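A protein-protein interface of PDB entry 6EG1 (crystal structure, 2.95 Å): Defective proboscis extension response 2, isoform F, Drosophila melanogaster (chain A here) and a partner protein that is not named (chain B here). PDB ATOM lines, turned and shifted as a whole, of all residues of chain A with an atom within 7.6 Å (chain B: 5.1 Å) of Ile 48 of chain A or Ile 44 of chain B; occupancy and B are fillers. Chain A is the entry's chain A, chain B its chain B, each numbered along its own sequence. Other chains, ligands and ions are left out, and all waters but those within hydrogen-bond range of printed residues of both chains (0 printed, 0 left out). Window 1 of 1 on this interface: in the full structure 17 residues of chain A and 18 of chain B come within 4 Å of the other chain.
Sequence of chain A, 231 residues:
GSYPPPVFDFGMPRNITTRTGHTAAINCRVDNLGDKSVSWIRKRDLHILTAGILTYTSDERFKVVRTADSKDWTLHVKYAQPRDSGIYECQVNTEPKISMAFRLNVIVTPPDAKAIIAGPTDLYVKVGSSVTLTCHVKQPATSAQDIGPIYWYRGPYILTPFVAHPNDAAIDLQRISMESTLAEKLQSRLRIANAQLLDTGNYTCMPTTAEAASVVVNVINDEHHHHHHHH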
ATOM      1  N   VAL A  38      -4.815   4.675  30.611  1.00  0.00           N
ATOM      2  CA  VAL A  38      -4.596   3.600  31.569  1.00  0.00           C
ATOM      3  C   VAL A  38      -4.309   2.328  30.788  1.00  0.00           C
ATOM      4  O   VAL A  38      -4.999   2.021  29.808  1.00  0.00           O
ATOM      5  CB  VAL A  38      -5.803   3.418  32.507  1.00  0.00           C
ATOM      6  CG1 VAL A  38      -5.621   2.186  33.377  1.00  0.00           C
ATOM      7  CG2 VAL A  38      -5.978   4.649  33.374  1.00  0.00           C
ATOM      8  N   SER A  39      -3.283   1.602  31.208  1.00  0.00           N
ATOM      9  CA  SER A  39      -2.884   0.367  30.557  1.00  0.00           C
ATOM     10  C   SER A  39      -2.932  -0.766  31.564  1.00  0.00           C
ATOM     11  O   SER A  39      -2.613  -0.577  32.743  1.00  0.00           O
ATOM     12  CB  SER A  39      -1.482   0.485  29.970  1.00  0.00           C
ATOM     13  OG  SER A  39      -1.363   1.668  29.204  1.00  0.00           O
ATOM     14  N   TRP A  40      -3.348  -1.937  31.101  1.00  0.00           N
ATOM     15  CA  TRP A  40      -3.300  -3.156  31.892  1.00  0.00           C
ATOM     16  C   TRP A  40      -2.209  -4.054  31.338  1.00  0.00           C
ATOM     17  O   TRP A  40      -2.204  -4.367  30.142  1.00  0.00           O
ATOM     18  CB  TRP A  40      -4.643  -3.879  31.882  1.00  0.00           C
ATOM     19  CG  TRP A  40      -5.633  -3.266  32.793  1.00  0.00           C
ATOM     20  CD1 TRP A  40      -6.651  -2.426  32.454  1.00  0.00           C
ATOM     21  CD2 TRP A  40      -5.707  -3.438  34.209  1.00  0.00           C
ATOM     22  NE1 TRP A  40      -7.360  -2.068  33.573  1.00  0.00           N
ATOM     23  CE2 TRP A  40      -6.799  -2.676  34.666  1.00  0.00           C
ATOM     24  CE3 TRP A  40      -4.957  -4.165  35.137  1.00  0.00           C
ATOM     25  CZ2 TRP A  40      -7.158  -2.619  36.008  1.00  0.00           C
ATOM     26  CZ3 TRP A  40      -5.313  -4.107  36.469  1.00  0.00           C
ATOM     27  CH2 TRP A  40      -6.405  -3.339  36.894  1.00  0.00           C
ATOM     28  N   ILE A  41      -1.292  -4.466  32.205  1.00  0.00           N
ATOM     29  CA  ILE A  41      -0.145  -5.267  31.807  1.00  0.00           C
ATOM     30  C   ILE A  41       0.004  -6.426  32.783  1.00  0.00           C
ATOM     31  O   ILE A  41      -0.334  -6.317  33.966  1.00  0.00           O
ATOM     32  CB  ILE A  41       1.139  -4.409  31.750  1.00  0.00           C
ATOM     33  CG1 ILE A  41       2.223  -5.109  30.941  1.00  0.00           C
ATOM     34  CG2 ILE A  41       1.659  -4.111  33.144  1.00  0.00           C
ATOM     35  CD1 ILE A  41       3.486  -4.288  30.823  1.00  0.00           C
ATOM     36  N   ARG A  42       0.495  -7.552  32.274  1.00  0.00           N
ATOM     37  CA  ARG A  42       0.768  -8.722  33.102  1.00  0.00           C
ATOM     38  C   ARG A  42       2.227  -8.660  33.543  1.00  0.00           C
ATOM     39  O   ARG A  42       3.137  -8.791  32.719  1.00  0.00           O
ATOM     40  CB  ARG A  42       0.466 -10.008  32.335  1.00  0.00           C
ATOM     41  CG  ARG A  42       0.670 -11.275  33.152  1.00  0.00           C
ATOM     42  CD  ARG A  42       0.011 -12.476  32.496  1.00  0.00           C
ATOM     43  NE  ARG A  42       0.572 -12.759  31.179  1.00  0.00           N
ATOM     44  CZ  ARG A  42       0.057 -13.630  30.318  1.00  0.00           C
ATOM     45  NH1 ARG A  42      -1.040 -14.303  30.636  1.00  0.00           N
ATOM     46  NH2 ARG A  42       0.633 -13.821  29.140  1.00  0.00           N
ATOM     47  N   ASP A  45       5.246 -11.531  32.647  1.00  0.00           N
ATOM     48  CA  ASP A  45       5.956 -11.597  31.380  1.00  0.00           C
ATOM     49  C   ASP A  45       5.906 -10.302  30.581  1.00  0.00           C
ATOM     50  O   ASP A  45       6.376 -10.286  29.438  1.00  0.00           O
ATOM     51  CB  ASP A  45       5.391 -12.735  30.513  1.00  0.00           C
ATOM     52  CG  ASP A  45       3.900 -12.587  30.245  1.00  0.00           C
ATOM     53  OD1 ASP A  45       3.179 -12.096  31.138  1.00  0.00           O
ATOM     54  OD2 ASP A  45       3.442 -12.966  29.145  1.00  0.00           O
ATOM     55  N   LEU A  46       5.346  -9.226  31.138  1.00  0.00           N
ATOM     56  CA  LEU A  46       5.204  -7.941  30.459  1.00  0.00           C
ATOM     57  C   LEU A  46       4.197  -7.979  29.318  1.00  0.00           C
ATOM     58  O   LEU A  46       4.205  -7.093  28.458  1.00  0.00           O
ATOM     59  CB  LEU A  46       6.546  -7.436  29.927  1.00  0.00           C
ATOM     60  CG  LEU A  46       7.509  -6.807  30.929  1.00  0.00           C
ATOM     61  CD1 LEU A  46       7.797  -7.753  32.080  1.00  0.00           C
ATOM     62  CD2 LEU A  46       8.787  -6.436  30.210  1.00  0.00           C
ATOM     63  N   HIS A  47       3.329  -8.985  29.275  1.00  0.00           N
ATOM     64  CA  HIS A  47       2.325  -9.035  28.222  1.00  0.00           C
ATOM     65  C   HIS A  47       1.362  -7.868  28.381  1.00  0.00           C
ATOM     66  O   HIS A  47       0.660  -7.761  29.390  1.00  0.00           O
ATOM     67  CB  HIS A  47       1.571 -10.361  28.269  1.00  0.00           C
ATOM     68  CG  HIS A  47       0.642 -10.572  27.112  1.00  0.00           C
ATOM     69  ND1 HIS A  47       0.731  -9.849  25.941  1.00  0.00           N
ATOM     70  CD2 HIS A  47      -0.393 -11.429  26.946  1.00  0.00           C
ATOM     71  CE1 HIS A  47      -0.211 -10.251  25.106  1.00  0.00           C
ATOM     72  NE2 HIS A  47      -0.906 -11.209  25.691  1.00  0.00           N
ATOM     73  N   ILE A  48       1.344  -6.979  27.391  1.00  0.00           N
ATOM     74  CA  ILE A  48       0.403  -5.870  27.415  1.00  0.00           C
ATOM     75  C   ILE A  48      -1.002  -6.405  27.185  1.00  0.00           C
ATOM     76  O   ILE A  48      -1.259  -7.124  26.211  1.00  0.00           O
ATOM     77  CB  ILE A  48       0.785  -4.823  26.362  1.00  0.00           C
ATOM     78  CG1 ILE A  48       2.202  -4.322  26.626  1.00  0.00           C
ATOM     79  CG2 ILE A  48      -0.200  -3.671  26.385  1.00  0.00           C
ATOM     80  CD1 ILE A  48       2.700  -3.362  25.596  1.00  0.00           C
ATOM     81  N   LEU A  49      -1.919  -6.071  28.088  1.00  0.00           N
ATOM     82  CA  LEU A  49      -3.293  -6.531  27.939  1.00  0.00           C
ATOM     83  C   LEU A  49      -4.159  -5.495  27.234  1.00  0.00           C
ATOM     84  O   LEU A  49      -4.797  -5.799  26.222  1.00  0.00           O
ATOM     85  CB  LEU A  49      -3.882  -6.886  29.305  1.00  0.00           C
ATOM     86  CG  LEU A  49      -3.180  -8.048  30.010  1.00  0.00           C
ATOM     87  CD1 LEU A  49      -3.850  -8.378  31.336  1.00  0.00           C
ATOM     88  CD2 LEU A  49      -3.132  -9.274  29.108  1.00  0.00           C
ATOM     89  N   THR A  50      -4.185  -4.270  27.746  1.00  0.00           N
ATOM     90  CA  THR A  50      -4.982  -3.213  27.142  1.00  0.00           C
ATOM     91  C   THR A  50      -4.249  -1.892  27.306  1.00  0.00           C
ATOM     92  O   THR A  50      -3.621  -1.645  28.340  1.00  0.00           O
ATOM     93  CB  THR A  50      -6.382  -3.125  27.766  1.00  0.00           C
ATOM     94  OG1 THR A  50      -6.272  -2.906  29.179  1.00  0.00           O
ATOM     95  CG2 THR A  50      -7.164  -4.411  27.520  1.00  0.00           C
ATOM     96  N   ALA A  51      -4.321  -1.057  26.276  1.00  0.00           N
ATOM     97  CA  ALA A  51      -3.770   0.292  26.312  1.00  0.00           C
ATOM     98  C   ALA A  51      -4.909   1.258  26.019  1.00  0.00           C
ATOM     99  O   ALA A  51      -5.349   1.374  24.869  1.00  0.00           O
ATOM    100  CB  ALA A  51      -2.632   0.454  25.308  1.00  0.00           C
ATOM    101  N   GLY A  52      -5.381   1.945  27.050  1.00  0.00           N
ATOM    102  CA  GLY A  52      -6.567   2.765  26.873  1.00  0.00           C
ATOM    103  C   GLY A  52      -7.761   1.855  26.699  1.00  0.00           C
ATOM    104  O   GLY A  52      -7.912   0.860  27.415  1.00  0.00           O
ATOM    105  N   LEU A  54      -8.176   0.437  23.691  1.00  0.00           N
ATOM    106  CA  LEU A  54      -7.672  -0.537  22.733  1.00  0.00           C
ATOM    107  C   LEU A  54      -7.198  -1.792  23.456  1.00  0.00           C
ATOM    108  O   LEU A  54      -6.481  -1.711  24.459  1.00  0.00           O
ATOM    109  CB  LEU A  54      -6.530   0.081  21.925  1.00  0.00           C
ATOM    110  CG  LEU A  54      -5.904  -0.698  20.766  1.00  0.00           C
ATOM    111  CD1 LEU A  54      -5.067   0.247  19.912  1.00  0.00           C
ATOM    112  CD2 LEU A  54      -5.057  -1.877  21.250  1.00  0.00           C
ATOM    113  N   THR A  55      -7.600  -2.954  22.952  1.00  0.00           N
ATOM    114  CA  THR A  55      -7.148  -4.232  23.487  1.00  0.00           C
ATOM    115  C   THR A  55      -5.969  -4.717  22.653  1.00  0.00           C
ATOM    116  O   THR A  55      -6.100  -4.904  21.439  1.00  0.00           O
ATOM    117  CB  THR A  55      -8.266  -5.273  23.480  1.00  0.00           C
ATOM    118  OG1 THR A  55      -9.329  -4.852  24.346  1.00  0.00           O
ATOM    119  CG2 THR A  55      -7.733  -6.613  23.960  1.00  0.00           C
ATOM    120  N   TYR A  56      -4.821  -4.910  23.303  1.00  0.00           N
ATOM    121  CA  TYR A  56      -3.627  -5.362  22.601  1.00  0.00           C
ATOM    122  C   TYR A  56      -3.538  -6.881  22.569  1.00  0.00           C
ATOM    123  O   TYR A  56      -3.334  -7.472  21.503  1.00  0.00           O
ATOM    124  CB  TYR A  56      -2.372  -4.773  23.251  1.00  0.00           C
ATOM    125  CG  TYR A  56      -1.081  -5.254  22.625  1.00  0.00           C
ATOM    126  CD1 TYR A  56      -0.586  -4.664  21.471  1.00  0.00           C
ATOM    127  CD2 TYR A  56      -0.357  -6.300  23.187  1.00  0.00           C
ATOM    128  CE1 TYR A  56       0.588  -5.098  20.893  1.00  0.00           C
ATOM    129  CE2 TYR A  56       0.820  -6.742  22.615  1.00  0.00           C
ATOM    130  CZ  TYR A  56       1.287  -6.136  21.467  1.00  0.00           C
ATOM    131  OH  TYR A  56       2.456  -6.563  20.886  1.00  0.00           O
ATOM    132  N   THR A  57      -3.693  -7.516  23.725  1.00  0.00           N
ATOM    133  CA  THR A  57      -3.614  -8.965  23.783  1.00  0.00           C
ATOM    134  C   THR A  57      -4.606  -9.578  22.808  1.00  0.00           C
ATOM    135  O   THR A  57      -5.599  -8.957  22.425  1.00  0.00           O
ATOM    136  CB  THR A  57      -3.894  -9.456  25.203  1.00  0.00           C
ATOM    137  OG1 THR A  57      -3.851 -10.888  25.228  1.00  0.00           O
ATOM    138  CG2 THR A  57      -5.261  -8.989  25.655  1.00  0.00           C
ATOM    139  N   SER A  58      -4.314 -10.805  22.387  1.00  0.00           N
ATOM    140  CA  SER A  58      -5.176 -11.529  21.465  1.00  0.00           C
ATOM    141  C   SER A  58      -5.890 -12.695  22.136  1.00  0.00           C
ATOM    142  O   SER A  58      -6.662 -13.399  21.477  1.00  0.00           O
ATOM    143  CB  SER A  58      -4.368 -12.012  20.253  1.00  0.00           C
ATOM    144  OG  SER A  58      -3.347 -12.915  20.640  1.00  0.00           O
ATOM    145  N   PHE A  62      -9.779 -11.528  27.515  1.00  0.00           N
ATOM    146  CA  PHE A  62      -9.313 -10.314  28.177  1.00  0.00           C
ATOM    147  C   PHE A  62      -9.933  -9.096  27.507  1.00  0.00           C
ATOM    148  O   PHE A  62      -9.796  -8.911  26.292  1.00  0.00           O
ATOM    149  CB  PHE A  62      -7.788 -10.223  28.138  1.00  0.00           C
ATOM    150  CG  PHE A  62      -7.102 -11.182  29.062  1.00  0.00           C
ATOM    151  CD1 PHE A  62      -6.801 -12.467  28.648  1.00  0.00           C
ATOM    152  CD2 PHE A  62      -6.759 -10.798  30.347  1.00  0.00           C
ATOM    153  CE1 PHE A  62      -6.174 -13.355  29.500  1.00  0.00           C
ATOM    154  CE2 PHE A  62      -6.132 -11.679  31.201  1.00  0.00           C
ATOM    155  CZ  PHE A  62      -5.840 -12.961  30.776  1.00  0.00           C
ATOM    156  N   GLU A  89      -0.865  -5.166  36.534  1.00  0.00           N
ATOM    157  CA  GLU A  89      -0.491  -3.791  36.829  1.00  0.00           C
ATOM    158  C   GLU A  89      -1.417  -2.838  36.092  1.00  0.00           C
ATOM    159  O   GLU A  89      -1.548  -2.920  34.868  1.00  0.00           O
ATOM    160  CB  GLU A  89       0.958  -3.514  36.431  1.00  0.00           C
ATOM    161  CG  GLU A  89       1.915  -3.354  37.598  1.00  0.00           C
ATOM    162  CD  GLU A  89       3.231  -2.720  37.178  1.00  0.00           C
ATOM    163  OE1 GLU A  89       3.220  -1.866  36.259  1.00  0.00           O
ATOM    164  OE2 GLU A  89       4.275  -3.080  37.763  1.00  0.00           O
ATOM    165  N   GLN A  91      -1.784   0.914  34.895  1.00  0.00           N
ATOM    166  CA  GLN A  91      -0.666   1.760  34.492  1.00  0.00           C
ATOM    167  C   GLN A  91      -1.163   3.028  33.815  1.00  0.00           C
ATOM    168  O   GLN A  91      -1.950   2.959  32.866  1.00  0.00           O
ATOM    169  CB  GLN A  91       0.258   0.972  33.558  1.00  0.00           C
ATOM    170  CG  GLN A  91       1.534   1.661  33.168  1.00  0.00           C
ATOM    171  CD  GLN A  91       2.457   0.722  32.427  1.00  0.00           C
ATOM    172  OE1 GLN A  91       2.958   1.042  31.350  1.00  0.00           O
ATOM    173  NE2 GLN A  91       2.679  -0.455  33.000  1.00  0.00           N
ATOM    174  N   ASN A  93       0.032   6.553  31.816  1.00  0.00           N
ATOM    175  CA  ASN A  93       1.165   6.831  30.939  1.00  0.00           C
ATOM    176  C   ASN A  93       1.821   8.168  31.244  1.00  0.00           C
ATOM    177  O   ASN A  93       2.266   8.871  30.328  1.00  0.00           O
ATOM    178  CB  ASN A  93       0.727   6.810  29.476  1.00  0.00           C
ATOM    179  CG  ASN A  93      -0.280   7.887  29.161  1.00  0.00           C
ATOM    180  OD1 ASN A  93      -0.871   8.472  30.066  1.00  0.00           O
ATOM    181  ND2 ASN A  93      -0.494   8.150  27.877  1.00  0.00           N
ATOM    182  N   THR A  94       1.873   8.543  32.517  1.00  0.00           N
ATOM    183  CA  THR A  94       2.625   9.726  32.897  1.00  0.00           C
ATOM    184  C   THR A  94       4.121   9.446  32.753  1.00  0.00           C
ATOM    185  O   THR A  94       4.550   8.331  32.447  1.00  0.00           O
ATOM    186  CB  THR A  94       2.275  10.152  34.321  1.00  0.00           C
ATOM    187  OG1 THR A  94       2.609   9.099  35.233  1.00  0.00           O
ATOM    188  CG2 THR A  94       0.784  10.468  34.432  1.00  0.00           C
ATOM    189  N   LYS A  97       6.042   6.875  34.748  1.00  0.00           N
ATOM    190  CA  LYS A  97       4.728   6.249  34.792  1.00  0.00           C
ATOM    191  C   LYS A  97       4.426   5.756  36.201  1.00  0.00           C
ATOM    192  O   LYS A  97       5.273   5.132  36.847  1.00  0.00           O
ATOM    193  CB  LYS A  97       4.649   5.094  33.791  1.00  0.00           C
ATOM    194  CG  LYS A  97       5.541   3.899  34.106  1.00  0.00           C
ATOM    195  CD  LYS A  97       4.819   2.852  34.953  1.00  0.00           C
ATOM    196  CE  LYS A  97       5.699   1.624  35.171  1.00  0.00           C
ATOM    197  NZ  LYS A  97       5.004   0.527  35.900  1.00  0.00           N
ATOM    198  N   ALA B  35       4.719  -3.839  19.671  1.00  0.00           N
ATOM    199  CA  ALA B  35       4.747  -2.954  20.828  1.00  0.00           C
ATOM    200  C   ALA B  35       6.149  -2.887  21.414  1.00  0.00           C
ATOM    201  O   ALA B  35       6.800  -3.920  21.599  1.00  0.00           O
ATOM    202  CB  ALA B  35       3.755  -3.421  21.900  1.00  0.00           C
ATOM    203  N   TRP B  36       6.606  -1.673  21.701  1.00  0.00           N
ATOM    204  CA  TRP B  36       7.859  -1.425  22.399  1.00  0.00           C
ATOM    205  C   TRP B  36       7.586  -1.156  23.872  1.00  0.00           C
ATOM    206  O   TRP B  36       6.507  -0.687  24.241  1.00  0.00           O
ATOM    207  CB  TRP B  36       8.598  -0.225  21.800  1.00  0.00           C
ATOM    208  CG  TRP B  36       9.316  -0.515  20.533  1.00  0.00           C
ATOM    209  CD1 TRP B  36       8.838  -0.370  19.266  1.00  0.00           C
ATOM    210  CD2 TRP B  36      10.658  -0.999  20.405  1.00  0.00           C
ATOM    211  NE1 TRP B  36       9.798  -0.737  18.353  1.00  0.00           N
ATOM    212  CE2 TRP B  36      10.925  -1.126  19.028  1.00  0.00           C
ATOM    213  CE3 TRP B  36      11.658  -1.338  21.321  1.00  0.00           C
ATOM    214  CZ2 TRP B  36      12.151  -1.576  18.546  1.00  0.00           C
ATOM    215  CZ3 TRP B  36      12.874  -1.785  20.840  1.00  0.00           C
ATOM    216  CH2 TRP B  36      13.109  -1.901  19.465  1.00  0.00           C
ATOM    217  N   LEU B  37       8.573  -1.447  24.715  1.00  0.00           N
ATOM    218  CA  LEU B  37       8.449  -1.049  26.109  1.00  0.00           C
ATOM    219  C   LEU B  37       9.782  -1.227  26.820  1.00  0.00           C
ATOM    220  O   LEU B  37      10.640  -2.004  26.395  1.00  0.00           O
ATOM    221  CB  LEU B  37       7.337  -1.821  26.829  1.00  0.00           C
ATOM    222  CG  LEU B  37       7.222  -3.338  26.797  1.00  0.00           C
ATOM    223  CD1 LEU B  37       6.112  -3.752  27.748  1.00  0.00           C
ATOM    224  CD2 LEU B  37       6.916  -3.821  25.399  1.00  0.00           C
ATOM    225  N   GLN B  42       8.932  -1.718  33.373  1.00  0.00           N
ATOM    226  CA  GLN B  42       7.723  -2.259  32.757  1.00  0.00           C
ATOM    227  C   GLN B  42       6.814  -1.131  32.269  1.00  0.00           C
ATOM    228  O   GLN B  42       5.649  -1.016  32.648  1.00  0.00           O
ATOM    229  CB  GLN B  42       6.994  -3.190  33.724  1.00  0.00           C
ATOM    230  CG  GLN B  42       7.785  -4.435  34.046  1.00  0.00           C
ATOM    231  CD  GLN B  42       7.023  -5.395  34.928  1.00  0.00           C
ATOM    232  OE1 GLN B  42       5.939  -5.079  35.421  1.00  0.00           O
ATOM    233  NE2 GLN B  42       7.587  -6.581  35.132  1.00  0.00           N
ATOM    234  N   THR B  43       7.381  -0.293  31.408  1.00  0.00           N
ATOM    235  CA  THR B  43       6.712   0.893  30.894  1.00  0.00           C
ATOM    236  C   THR B  43       6.361   0.666  29.433  1.00  0.00           C
ATOM    237  O   THR B  43       7.252   0.466  28.603  1.00  0.00           O
ATOM    238  CB  THR B  43       7.603   2.126  31.043  1.00  0.00           C
ATOM    239  OG1 THR B  43       7.862   2.368  32.431  1.00  0.00           O
ATOM    240  CG2 THR B  43       6.935   3.349  30.427  1.00  0.00           C
ATOM    241  N   ILE B  44       5.065   0.702  29.118  1.00  0.00           N
ATOM    242  CA  ILE B  44       4.648   0.617  27.724  1.00  0.00           C
ATOM    243  C   ILE B  44       5.138   1.853  26.989  1.00  0.00           C
ATOM    244  O   ILE B  44       4.882   2.988  27.407  1.00  0.00           O
ATOM    245  CB  ILE B  44       3.122   0.475  27.624  1.00  0.00           C
ATOM    246  CG1 ILE B  44       2.651  -0.791  28.337  1.00  0.00           C
ATOM    247  CG2 ILE B  44       2.686   0.446  26.171  1.00  0.00           C
ATOM    248  CD1 ILE B  44       1.158  -0.935  28.359  1.00  0.00           C
ATOM    249  N   LEU B  45       5.854   1.641  25.886  1.00  0.00           N
ATOM    250  CA  LEU B  45       6.384   2.747  25.097  1.00  0.00           C
ATOM    251  C   LEU B  45       5.497   3.074  23.900  1.00  0.00           C
ATOM    252  O   LEU B  45       4.962   4.182  23.807  1.00  0.00           O
ATOM    253  CB  LEU B  45       7.813   2.434  24.639  1.00  0.00           C
ATOM    254  CG  LEU B  45       8.833   2.400  25.774  1.00  0.00           C
ATOM    255  CD1 LEU B  45      10.256   2.415  25.230  1.00  0.00           C
ATOM    256  CD2 LEU B  45       8.590   3.565  26.714  1.00  0.00           C
ATOM    257  N   THR B  46       5.329   2.127  22.980  1.00  0.00           N
ATOM    258  CA  THR B  46       4.527   2.356  21.790  1.00  0.00           C
ATOM    259  C   THR B  46       3.788   1.083  21.407  1.00  0.00           C
ATOM    260  O   THR B  46       4.205  -0.031  21.735  1.00  0.00           O
ATOM    261  CB  THR B  46       5.381   2.820  20.604  1.00  0.00           C
ATOM    262  OG1 THR B  46       6.336   1.802  20.277  1.00  0.00           O
ATOM    263  CG2 THR B  46       6.108   4.107  20.944  1.00  0.00           C
ATOM    264  N   ILE B  47       2.679   1.269  20.698  1.00  0.00           N
ATOM    265  CA  ILE B  47       1.899   0.179  20.127  1.00  0.00           C
ATOM    266  C   ILE B  47       1.565   0.565  18.696  1.00  0.00           C
ATOM    267  O   ILE B  47       1.030   1.652  18.453  1.00  0.00           O
ATOM    268  CB  ILE B  47       0.621  -0.104  20.940  1.00  0.00           C
ATOM    269  CG1 ILE B  47       0.979  -0.412  22.396  1.00  0.00           C
ATOM    270  CG2 ILE B  47      -0.156  -1.262  20.337  1.00  0.00           C
ATOM    271  CD1 ILE B  47      -0.146  -1.036  23.191  1.00  0.00           C
ATOM    272  N   ILE B  52       2.465   5.477  23.452  1.00  0.00           N
ATOM    273  CA  ILE B  52       1.680   5.480  24.680  1.00  0.00           C
ATOM    274  C   ILE B  52       2.320   6.379  25.728  1.00  0.00           C
ATOM    275  O   ILE B  52       1.620   7.043  26.501  1.00  0.00           O
ATOM    276  CB  ILE B  52       1.491   4.046  25.206  1.00  0.00           C
ATOM    277  CG1 ILE B  52       0.266   3.399  24.564  1.00  0.00           C
ATOM    278  CG2 ILE B  52       1.358   4.043  26.715  1.00  0.00           C
ATOM    279  CD1 ILE B  52       0.406   3.189  23.079  1.00  0.00           C
ATOM    280  N   THR B  53       3.649   6.424  25.773  1.00  0.00           N
ATOM    281  CA  THR B  53       4.323   7.223  26.785  1.00  0.00           C
ATOM    282  C   THR B  53       4.213   8.710  26.466  1.00  0.00           C
ATOM    283  O   THR B  53       4.263   9.120  25.303  1.00  0.00           O
ATOM    284  CB  THR B  53       5.793   6.822  26.894  1.00  0.00           C
ATOM    285  OG1 THR B  53       6.378   7.474  28.026  1.00  0.00           O
ATOM    286  CG2 THR B  53       6.552   7.225  25.638  1.00  0.00           C
ATOM    287  N   GLN B  86       7.528  -6.607  21.370  1.00  0.00           N
ATOM    288  CA  GLN B  86       6.486  -7.577  21.674  1.00  0.00           C
ATOM    289  C   GLN B  86       5.501  -7.671  20.518  1.00  0.00           C
ATOM    290  O   GLN B  86       5.179  -6.666  19.878  1.00  0.00           O
ATOM    291  CB  GLN B  86       5.755  -7.193  22.967  1.00  0.00           C
ATOM    292  CG  GLN B  86       4.743  -8.210  23.454  1.00  0.00           C
ATOM    293  CD  GLN B  86       4.230  -7.895  24.850  1.00  0.00           C
ATOM    294  OE1 GLN B  86       3.032  -7.982  25.122  1.00  0.00           O
ATOM    295  NE2 GLN B  86       5.140  -7.530  25.743  1.00  0.00           N
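Ile 44 of chain B touches Ser 39 of chain A.
Leu 46 of chain A touches Leu 37 of chain B (O to CD1, 3.9 Å).
NE2 of Gln 42 of chain B touches CD1 of Leu 46 of chain A (3.3 Å).
Ala 35 of chain B touches Ile 48 of chain A (CB to CD1, 3.8 Å).
Ile 48 of chain A touches Ile 44 of chain B (CG2 to CD1, 3.6 Å).
Ala 51 of chain A touches Ile 47 of chain B (CB to CD1, 3.6 Å).
Ala 35 of chain B touches Tyr 56 of chain A (CB to OH, 3.5 Å).
Ile 47 of chain B touches Tyr 56 of chain A.
Lys 97 of chain A touches Gln 42 of chain B.
Lys 97 of chain A touches Thr 43 of chain B.
Asp 45 of chain A touches none of the printed residues of chain B.
Ile 48 of chain A touches just these residues of chain B: Ala 35 (3.8 Å), Ile 44 (3.6 Å) and Gln 86 (3.0 Å).
Gly 52 of chain A touches none of the printed residues of chain B.
Of the printed residues of chain B, Asn 93 of chain A touches Ile 52 (2.8 Å).
Printed residues of chain B within 4 Å of Lys 97 of chain A: Gln 42 and Thr 43.
Of the printed residues of chain A, Ala 35 of chain B touches Ile 48 and Tyr 56.
Ile 44 of chain B touches three residues of chain A.
Of the printed residues of chain A, Ile 52 of chain B touches Asn 93.
Of the printed residues of chain A, Gln 86 of chain B touches Leu 46, His 47, Ile 48 and Tyr 56.
The nearest residue of chain B that does not touch Ile 48 of chain A is Leu 37 of chain B (4.1 Å).
The nearest residue of chain A that does not touch Ile 44 of chain B is Ile 41 of chain A (4.4 Å).
Hydrophobic or aromatic side chains of chain A that line the printed part of chain B: Leu 46, His 47, Ile 48, Ala 51 and Tyr 56.
Hydrophobic or aromatic side chains of chain B that line the printed part of chain A: Ala 35, Leu 37, Ile 44, Ile 47 and Ile 52.
Among the printed residues, 19 pairs touch across the chains.
Among the printed residues, no Asp or Glu carboxylate lies within 4 Å of a Lys or Arg side-chain nitrogen of the other chain.
The backbone NH (N) of Glu 89 of chain A is in hydrogen-bond range of the backbone carbonyl oxygen (O) of Ile 41 of chain A.
The backbone NH of Arg 42 of chain A lies within hydrogen-bond range of the backbone carbonyl oxygen of His 47 of chain A, at 2.9 Å.
The backbone NH of Tyr 56 of chain A lies within hydrogen-bond range of the backbone carbonyl oxygen of Leu 49 of chain A, at 3.1 Å.
OE1 of Glu 89 of chain A lies within salt-bridge range of NZ of Lys 97 of chain A, at 3.0 Å.
N of Gln 86 of chain B lies within hydrogen-bond range of O of Ala 35 of chain B (2.8 Å).
O of Leu 45 of chain B lies within hydrogen-bond range of N of Ile 52 of chain B (2.8 Å).
The backbone carbonyl oxygen (O) of Leu 46 of chain A lies within hydrogen-bond range of the side-chain amide nitrogen (NE2) of Gln 86 of chain B (2.9 Å).
ND1 of His 47 of chain A is in hydrogen-bond range of OE1 of Gln 86 of chain B (3.1 Å).
N of Ile 48 of chain A lies within hydrogen-bond range of OE1 of Gln 86 of chain B (3.0 Å).
The side-chain hydroxyl (OH) of Tyr 56 of chain A lies within hydrogen-bond range of the backbone carbonyl oxygen (O) of Gln 86 of chain B (2.9 Å).
The side-chain carboxylate of Glu 89 of chain A lies close to the side-chain amide oxygen of Gln 42 of chain B (3.5 Å).
NE2 of Gln 91 of chain A lies within hydrogen-bond range of O of Gln 42 of chain B, at 3.0 Å.
The side-chain amide oxygen (OE1) of Gln 91 of chain A lies within hydrogen-bond range of the backbone NH (N) of Ile 44 of chain B (3.1 Å).
ND2 of Asn 93 of chain A sits at hydrogen-bond distance from O of Ile 52 of chain B, 2.8 Å away.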
